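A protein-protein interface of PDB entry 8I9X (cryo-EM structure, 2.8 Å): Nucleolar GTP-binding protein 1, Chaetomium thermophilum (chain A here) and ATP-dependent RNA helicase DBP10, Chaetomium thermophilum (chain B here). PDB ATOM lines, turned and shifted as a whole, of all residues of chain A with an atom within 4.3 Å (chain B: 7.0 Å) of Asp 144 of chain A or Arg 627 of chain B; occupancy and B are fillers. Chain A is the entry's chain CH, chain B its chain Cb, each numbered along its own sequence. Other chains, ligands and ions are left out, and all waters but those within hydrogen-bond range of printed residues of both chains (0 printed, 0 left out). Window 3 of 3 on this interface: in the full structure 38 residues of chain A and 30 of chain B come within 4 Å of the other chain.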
ATOM      1  N   LEU A 142     -19.430   5.415  23.815  1.00  0.00           N
ATOM      2  CA  LEU A 142     -20.295   6.331  23.073  1.00  0.00           C
ATOM      3  C   LEU A 142     -19.773   6.548  21.660  1.00  0.00           C
ATOM      4  O   LEU A 142     -19.695   7.665  21.157  1.00  0.00           O
ATOM      5  CB  LEU A 142     -20.407   7.660  23.806  1.00  0.00           C
ATOM      6  CG  LEU A 142     -21.508   7.860  24.839  1.00  0.00           C
ATOM      7  CD1 LEU A 142     -21.506   9.313  25.247  1.00  0.00           C
ATOM      8  CD2 LEU A 142     -22.861   7.452  24.295  1.00  0.00           C
ATOM      9  N   LYS A 143     -19.408   5.447  21.015  1.00  0.00           N
ATOM     10  CA  LYS A 143     -19.128   5.453  19.579  1.00  0.00           C
ATOM     11  C   LYS A 143     -20.396   5.599  18.735  1.00  0.00           C
ATOM     12  O   LYS A 143     -20.563   6.588  18.014  1.00  0.00           O
ATOM     13  CB  LYS A 143     -18.388   4.171  19.194  1.00  0.00           C
ATOM     14  CG  LYS A 143     -17.971   4.105  17.739  1.00  0.00           C
ATOM     15  CD  LYS A 143     -17.627   2.684  17.331  1.00  0.00           C
ATOM     16  CE  LYS A 143     -17.377   2.585  15.836  1.00  0.00           C
ATOM     17  NZ  LYS A 143     -18.647   2.590  15.058  1.00  0.00           N
ATOM     18  N   ASP A 144     -21.297   4.615  18.805  1.00  0.00           N
ATOM     19  CA  ASP A 144     -22.439   4.566  17.888  1.00  0.00           C
ATOM     20  C   ASP A 144     -23.413   5.732  18.043  1.00  0.00           C
ATOM     21  O   ASP A 144     -23.863   6.272  17.012  1.00  0.00           O
ATOM     22  CB  ASP A 144     -23.165   3.226  18.044  1.00  0.00           C
ATOM     23  CG  ASP A 144     -22.342   2.058  17.546  1.00  0.00           C
ATOM     24  OD1 ASP A 144     -21.522   2.256  16.626  1.00  0.00           O
ATOM     25  OD2 ASP A 144     -22.519   0.940  18.072  1.00  0.00           O
ATOM     26  N   PRO A 145     -23.810   6.148  19.254  1.00  0.00           N
ATOM     27  CA  PRO A 145     -24.716   7.304  19.354  1.00  0.00           C
ATOM     28  C   PRO A 145     -24.174   8.545  18.675  1.00  0.00           C
ATOM     29  O   PRO A 145     -24.949   9.349  18.152  1.00  0.00           O
ATOM     30  CB  PRO A 145     -24.857   7.499  20.867  1.00  0.00           C
ATOM     31  CG  PRO A 145     -24.623   6.176  21.433  1.00  0.00           C
ATOM     32  CD  PRO A 145     -23.592   5.527  20.573  1.00  0.00           C
ATOM     33  N   LEU A 146     -22.853   8.725  18.676  1.00  0.00           N
ATOM     34  CA  LEU A 146     -22.268   9.867  17.985  1.00  0.00           C
ATOM     35  C   LEU A 146     -22.529   9.794  16.485  1.00  0.00           C
ATOM     36  O   LEU A 146     -22.873  10.804  15.860  1.00  0.00           O
ATOM     37  CB  LEU A 146     -20.772   9.941  18.282  1.00  0.00           C
ATOM     38  CG  LEU A 146     -20.430  10.362  19.714  1.00  0.00           C
ATOM     39  CD1 LEU A 146     -18.929  10.476  19.919  1.00  0.00           C
ATOM     40  CD2 LEU A 146     -21.119  11.663  20.076  1.00  0.00           C
ATOM     41  N   ILE A 147     -22.388   8.605  15.893  1.00  0.00           N
ATOM     42  CA  ILE A 147     -22.677   8.439  14.469  1.00  0.00           C
ATOM     43  C   ILE A 147     -24.144   8.734  14.186  1.00  0.00           C
ATOM     44  O   ILE A 147     -24.480   9.476  13.246  1.00  0.00           O
ATOM     45  CB  ILE A 147     -22.286   7.021  14.010  1.00  0.00           C
ATOM     46  CG1 ILE A 147     -20.771   6.913  13.840  1.00  0.00           C
ATOM     47  CG2 ILE A 147     -22.993   6.660  12.719  1.00  0.00           C
ATOM     48  CD1 ILE A 147     -20.260   5.494  13.852  1.00  0.00           C
ATOM     49  N   TYR A 148     -25.040   8.172  15.001  1.00  0.00           N
ATOM     50  CA  TYR A 148     -26.466   8.396  14.786  1.00  0.00           C
ATOM     51  C   TYR A 148     -26.815   9.876  14.901  1.00  0.00           C
ATOM     52  O   TYR A 148     -27.548  10.421  14.063  1.00  0.00           O
ATOM     53  CB  TYR A 148     -27.279   7.562  15.778  1.00  0.00           C
ATOM     54  CG  TYR A 148     -28.751   7.899  15.809  1.00  0.00           C
ATOM     55  CD1 TYR A 148     -29.267   8.751  16.774  1.00  0.00           C
ATOM     56  CD2 TYR A 148     -29.624   7.376  14.868  1.00  0.00           C
ATOM     57  CE1 TYR A 148     -30.606   9.064  16.807  1.00  0.00           C
ATOM     58  CE2 TYR A 148     -30.966   7.684  14.893  1.00  0.00           C
ATOM     59  CZ  TYR A 148     -31.450   8.530  15.863  1.00  0.00           C
ATOM     60  OH  TYR A 148     -32.785   8.843  15.896  1.00  0.00           O
ATOM     61  N   LYS B 616     -20.704   2.608   6.725  1.00  0.00           N
ATOM     62  CA  LYS B 616     -20.391   2.395   8.133  1.00  0.00           C
ATOM     63  C   LYS B 616     -21.409   3.074   9.039  1.00  0.00           C
ATOM     64  O   LYS B 616     -21.776   2.521  10.081  1.00  0.00           O
ATOM     65  CB  LYS B 616     -18.984   2.900   8.447  1.00  0.00           C
ATOM     66  CG  LYS B 616     -17.878   2.127   7.753  1.00  0.00           C
ATOM     67  CD  LYS B 616     -16.511   2.666   8.134  1.00  0.00           C
ATOM     68  CE  LYS B 616     -15.401   1.867   7.475  1.00  0.00           C
ATOM     69  NZ  LYS B 616     -14.053   2.356   7.877  1.00  0.00           N
ATOM     70  N   ALA B 617     -21.870   4.269   8.664  1.00  0.00           N
ATOM     71  CA  ALA B 617     -22.901   4.943   9.445  1.00  0.00           C
ATOM     72  C   ALA B 617     -24.182   4.121   9.480  1.00  0.00           C
ATOM     73  O   ALA B 617     -24.805   3.964  10.535  1.00  0.00           O
ATOM     74  CB  ALA B 617     -23.165   6.336   8.875  1.00  0.00           C
ATOM     75  N   GLU B 619     -24.465   0.856   9.041  1.00  0.00           N
ATOM     76  CA  GLU B 619     -24.232  -0.343   9.841  1.00  0.00           C
ATOM     77  C   GLU B 619     -24.280  -0.029  11.331  1.00  0.00           C
ATOM     78  O   GLU B 619     -24.868  -0.785  12.114  1.00  0.00           O
ATOM     79  CB  GLU B 619     -22.889  -0.971   9.471  1.00  0.00           C
ATOM     80  CG  GLU B 619     -22.821  -1.501   8.051  1.00  0.00           C
ATOM     81  CD  GLU B 619     -21.397  -1.742   7.591  1.00  0.00           C
ATOM     82  OE1 GLU B 619     -20.462  -1.400   8.345  1.00  0.00           O
ATOM     83  OE2 GLU B 619     -21.214  -2.273   6.476  1.00  0.00           O
ATOM     84  N   ALA B 620     -23.661   1.081  11.741  1.00  0.00           N
ATOM     85  CA  ALA B 620     -23.695   1.474  13.145  1.00  0.00           C
ATOM     86  C   ALA B 620     -25.117   1.766  13.599  1.00  0.00           C
ATOM     87  O   ALA B 620     -25.522   1.356  14.693  1.00  0.00           O
ATOM     88  CB  ALA B 620     -22.796   2.687  13.375  1.00  0.00           C
ATOM     89  N   VAL B 621     -25.896   2.463  12.766  1.00  0.00           N
ATOM     90  CA  VAL B 621     -27.284   2.751  13.116  1.00  0.00           C
ATOM     91  C   VAL B 621     -28.080   1.462  13.258  1.00  0.00           C
ATOM     92  O   VAL B 621     -28.848   1.295  14.210  1.00  0.00           O
ATOM     93  CB  VAL B 621     -27.917   3.698  12.081  1.00  0.00           C
ATOM     94  CG1 VAL B 621     -29.406   3.849  12.344  1.00  0.00           C
ATOM     95  CG2 VAL B 621     -27.247   5.058  12.131  1.00  0.00           C
ATOM     96  N   ARG B 622     -27.905   0.525  12.322  1.00  0.00           N
ATOM     97  CA  ARG B 622     -28.653  -0.728  12.386  1.00  0.00           C
ATOM     98  C   ARG B 622     -28.291  -1.519  13.637  1.00  0.00           C
ATOM     99  O   ARG B 622     -29.170  -2.033  14.340  1.00  0.00           O
ATOM    100  CB  ARG B 622     -28.394  -1.561  11.129  1.00  0.00           C
ATOM    101  CG  ARG B 622     -29.185  -1.119   9.909  1.00  0.00           C
ATOM    102  CD  ARG B 622     -28.551  -1.638   8.629  1.00  0.00           C
ATOM    103  NE  ARG B 622     -29.437  -1.497   7.479  1.00  0.00           N
ATOM    104  CZ  ARG B 622     -29.056  -1.658   6.219  1.00  0.00           C
ATOM    105  NH1 ARG B 622     -27.809  -1.969   5.906  1.00  0.00           N
ATOM    106  NH2 ARG B 622     -29.953  -1.505   5.246  1.00  0.00           N
ATOM    107  N   SER B 623     -26.993  -1.619  13.935  1.00  0.00           N
ATOM    108  CA  SER B 623     -26.559  -2.354  15.117  1.00  0.00           C
ATOM    109  C   SER B 623     -27.077  -1.703  16.392  1.00  0.00           C
ATOM    110  O   SER B 623     -27.500  -2.396  17.327  1.00  0.00           O
ATOM    111  CB  SER B 623     -25.035  -2.449  15.144  1.00  0.00           C
ATOM    112  OG  SER B 623     -24.453  -1.177  15.374  1.00  0.00           O
ATOM    113  N   PHE B 624     -27.058  -0.370  16.450  1.00  0.00           N
ATOM    114  CA  PHE B 624     -27.523   0.321  17.645  1.00  0.00           C
ATOM    115  C   PHE B 624     -29.034   0.190  17.808  1.00  0.00           C
ATOM    116  O   PHE B 624     -29.531   0.056  18.935  1.00  0.00           O
ATOM    117  CB  PHE B 624     -27.084   1.784  17.590  1.00  0.00           C
ATOM    118  CG  PHE B 624     -27.023   2.447  18.932  1.00  0.00           C
ATOM    119  CD1 PHE B 624     -26.210   1.938  19.933  1.00  0.00           C
ATOM    120  CD2 PHE B 624     -27.742   3.599  19.183  1.00  0.00           C
ATOM    121  CE1 PHE B 624     -26.149   2.549  21.169  1.00  0.00           C
ATOM    122  CE2 PHE B 624     -27.678   4.218  20.412  1.00  0.00           C
ATOM    123  CZ  PHE B 624     -26.888   3.688  21.408  1.00  0.00           C
ATOM    124  N   ARG B 625     -29.782   0.199  16.700  1.00  0.00           N
ATOM    125  CA  ARG B 625     -31.222  -0.015  16.794  1.00  0.00           C
ATOM    126  C   ARG B 625     -31.517  -1.426  17.284  1.00  0.00           C
ATOM    127  O   ARG B 625     -32.408  -1.631  18.118  1.00  0.00           O
ATOM    128  CB  ARG B 625     -31.905   0.211  15.442  1.00  0.00           C
ATOM    129  CG  ARG B 625     -31.805   1.613  14.829  1.00  0.00           C
ATOM    130  CD  ARG B 625     -32.688   2.652  15.493  1.00  0.00           C
ATOM    131  NE  ARG B 625     -32.123   3.047  16.776  1.00  0.00           N
ATOM    132  CZ  ARG B 625     -31.103   3.882  16.915  1.00  0.00           C
ATOM    133  NH1 ARG B 625     -30.541   4.468  15.871  1.00  0.00           N
ATOM    134  NH2 ARG B 625     -30.633   4.135  18.132  1.00  0.00           N
ATOM    135  N   GLN B 626     -30.769  -2.413  16.778  1.00  0.00           N
ATOM    136  CA  GLN B 626     -30.927  -3.783  17.254  1.00  0.00           C
ATOM    137  C   GLN B 626     -30.601  -3.901  18.735  1.00  0.00           C
ATOM    138  O   GLN B 626     -31.273  -4.644  19.460  1.00  0.00           O
ATOM    139  CB  GLN B 626     -30.043  -4.726  16.439  1.00  0.00           C
ATOM    140  CG  GLN B 626     -30.559  -4.999  15.040  1.00  0.00           C
ATOM    141  CD  GLN B 626     -29.667  -5.949  14.270  1.00  0.00           C
ATOM    142  OE1 GLN B 626     -28.585  -6.317  14.731  1.00  0.00           O
ATOM    143  NE2 GLN B 626     -30.116  -6.356  13.089  1.00  0.00           N
ATOM    144  N   ARG B 627     -29.572  -3.191  19.199  1.00  0.00           N
ATOM    145  CA  ARG B 627     -29.255  -3.200  20.622  1.00  0.00           C
ATOM    146  C   ARG B 627     -30.366  -2.588  21.464  1.00  0.00           C
ATOM    147  O   ARG B 627     -30.723  -3.146  22.506  1.00  0.00           O
ATOM    148  CB  ARG B 627     -27.947  -2.457  20.888  1.00  0.00           C
ATOM    149  CG  ARG B 627     -26.692  -3.246  20.571  1.00  0.00           C
ATOM    150  CD  ARG B 627     -25.455  -2.433  20.909  1.00  0.00           C
ATOM    151  NE  ARG B 627     -24.234  -3.021  20.371  1.00  0.00           N
ATOM    152  CZ  ARG B 627     -23.033  -2.471  20.472  1.00  0.00           C
ATOM    153  NH1 ARG B 627     -22.853  -1.312  21.087  1.00  0.00           N
ATOM    154  NH2 ARG B 627     -21.985  -3.099  19.949  1.00  0.00           N
ATOM    155  N   ILE B 628     -30.923  -1.454  21.037  1.00  0.00           N
ATOM    156  CA  ILE B 628     -31.944  -0.765  21.820  1.00  0.00           C
ATOM    157  C   ILE B 628     -33.315  -1.424  21.666  1.00  0.00           C
ATOM    158  O   ILE B 628     -34.246  -1.090  22.407  1.00  0.00           O
ATOM    159  CB  ILE B 628     -32.000   0.726  21.454  1.00  0.00           C
ATOM    160  CG1 ILE B 628     -30.631   1.366  21.629  1.00  0.00           C
ATOM    161  CG2 ILE B 628     -32.941   1.498  22.375  1.00  0.00           C
ATOM    162  CD1 ILE B 628     -30.612   2.800  21.198  1.00  0.00           C
ATOM    163  N   GLY B 629     -33.452  -2.375  20.738  1.00  0.00           N
ATOM    164  CA  GLY B 629     -34.698  -3.081  20.522  1.00  0.00           C
ATOM    165  C   GLY B 629     -35.377  -3.507  21.809  1.00  0.00           C
ATOM    166  O   GLY B 629     -34.722  -3.812  22.810  1.00  0.00           O
ATOM    167  N   PRO B 630     -36.710  -3.527  21.804  1.00  0.00           N
ATOM    168  CA  PRO B 630     -37.457  -3.673  23.062  1.00  0.00           C
ATOM    169  C   PRO B 630     -37.126  -4.969  23.788  1.00  0.00           C
ATOM    170  O   PRO B 630     -36.897  -6.012  23.173  1.00  0.00           O
ATOM    171  CB  PRO B 630     -38.922  -3.640  22.609  1.00  0.00           C
ATOM    172  CG  PRO B 630     -38.883  -3.991  21.154  1.00  0.00           C
ATOM    173  CD  PRO B 630     -37.606  -3.405  20.642  1.00  0.00           C
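NH1 of Arg 627 of chain B lies within salt-bridge range of OD2 of Asp 144 of chain A (3.8 Å).
NZ of Lys 143 of chain A lies within salt-bridge range of OD1 of Asp 144 of chain A (3.3 Å). OG of Ser 623 of chain B lies within hydrogen-bond range of O of Glu 619 of chain B, at 3.3 Å. The backbone carbonyl oxygen (O) of Ala 620 of chain B lies within hydrogen-bond range of the side-chain hydroxyl (OG) of Ser 623 of chain B.
Among the printed residues, merely in contact across the chains: Asp 144 of chain A with Ala 620 of chain B, Asp 144 of chain A with Ser 623 of chain B, Asp 144 of chain A with Phe 624 of chain B, Pro 145 of chain A with Phe 624 of chain B, Ile 147 of chain A with Ala 617 of chain B, Ile 147 of chain A with Ala 620 of chain B and Tyr 148 of chain A with Arg 625 of chain B.
Asp 144 of chain A touches just these residues of chain B: Ala 620, Ser 623, Phe 624 and Arg 627. Of chain A, only Asp 144 (3.8 Å) comes within 4 Å of Arg 627 of chain B. Of the printed residues of chain A, Phe 624 of chain B touches Asp 144 (3.8 Å) and Pro 145 (3.4 Å). Of the printed residues of chain B, Ile 147 of chain A touches Ala 617 (3.7 Å) and Ala 620 (3.8 Å). Of the printed residues of chain A, Ser 623 of chain B touches Asp 144. Printed residues of chain B within 4 Å of Tyr 148 of chain A: Arg 625. Of the printed residues of chain A, Ala 617 of chain B touches Ile 147. Ile 628 of chain B touches none of the printed residues of chain A. Glu 619 of chain B touches none of the printed residues of chain A.
Of the 14 printed residues of chain B, 6 touch a printed residue of chain A. Among the printed residues, Asp or Glu carboxylates within 4 Å of a Lys or Arg side-chain nitrogen of the other chain: Asp 144 of chain A with Arg 627 of chain B.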
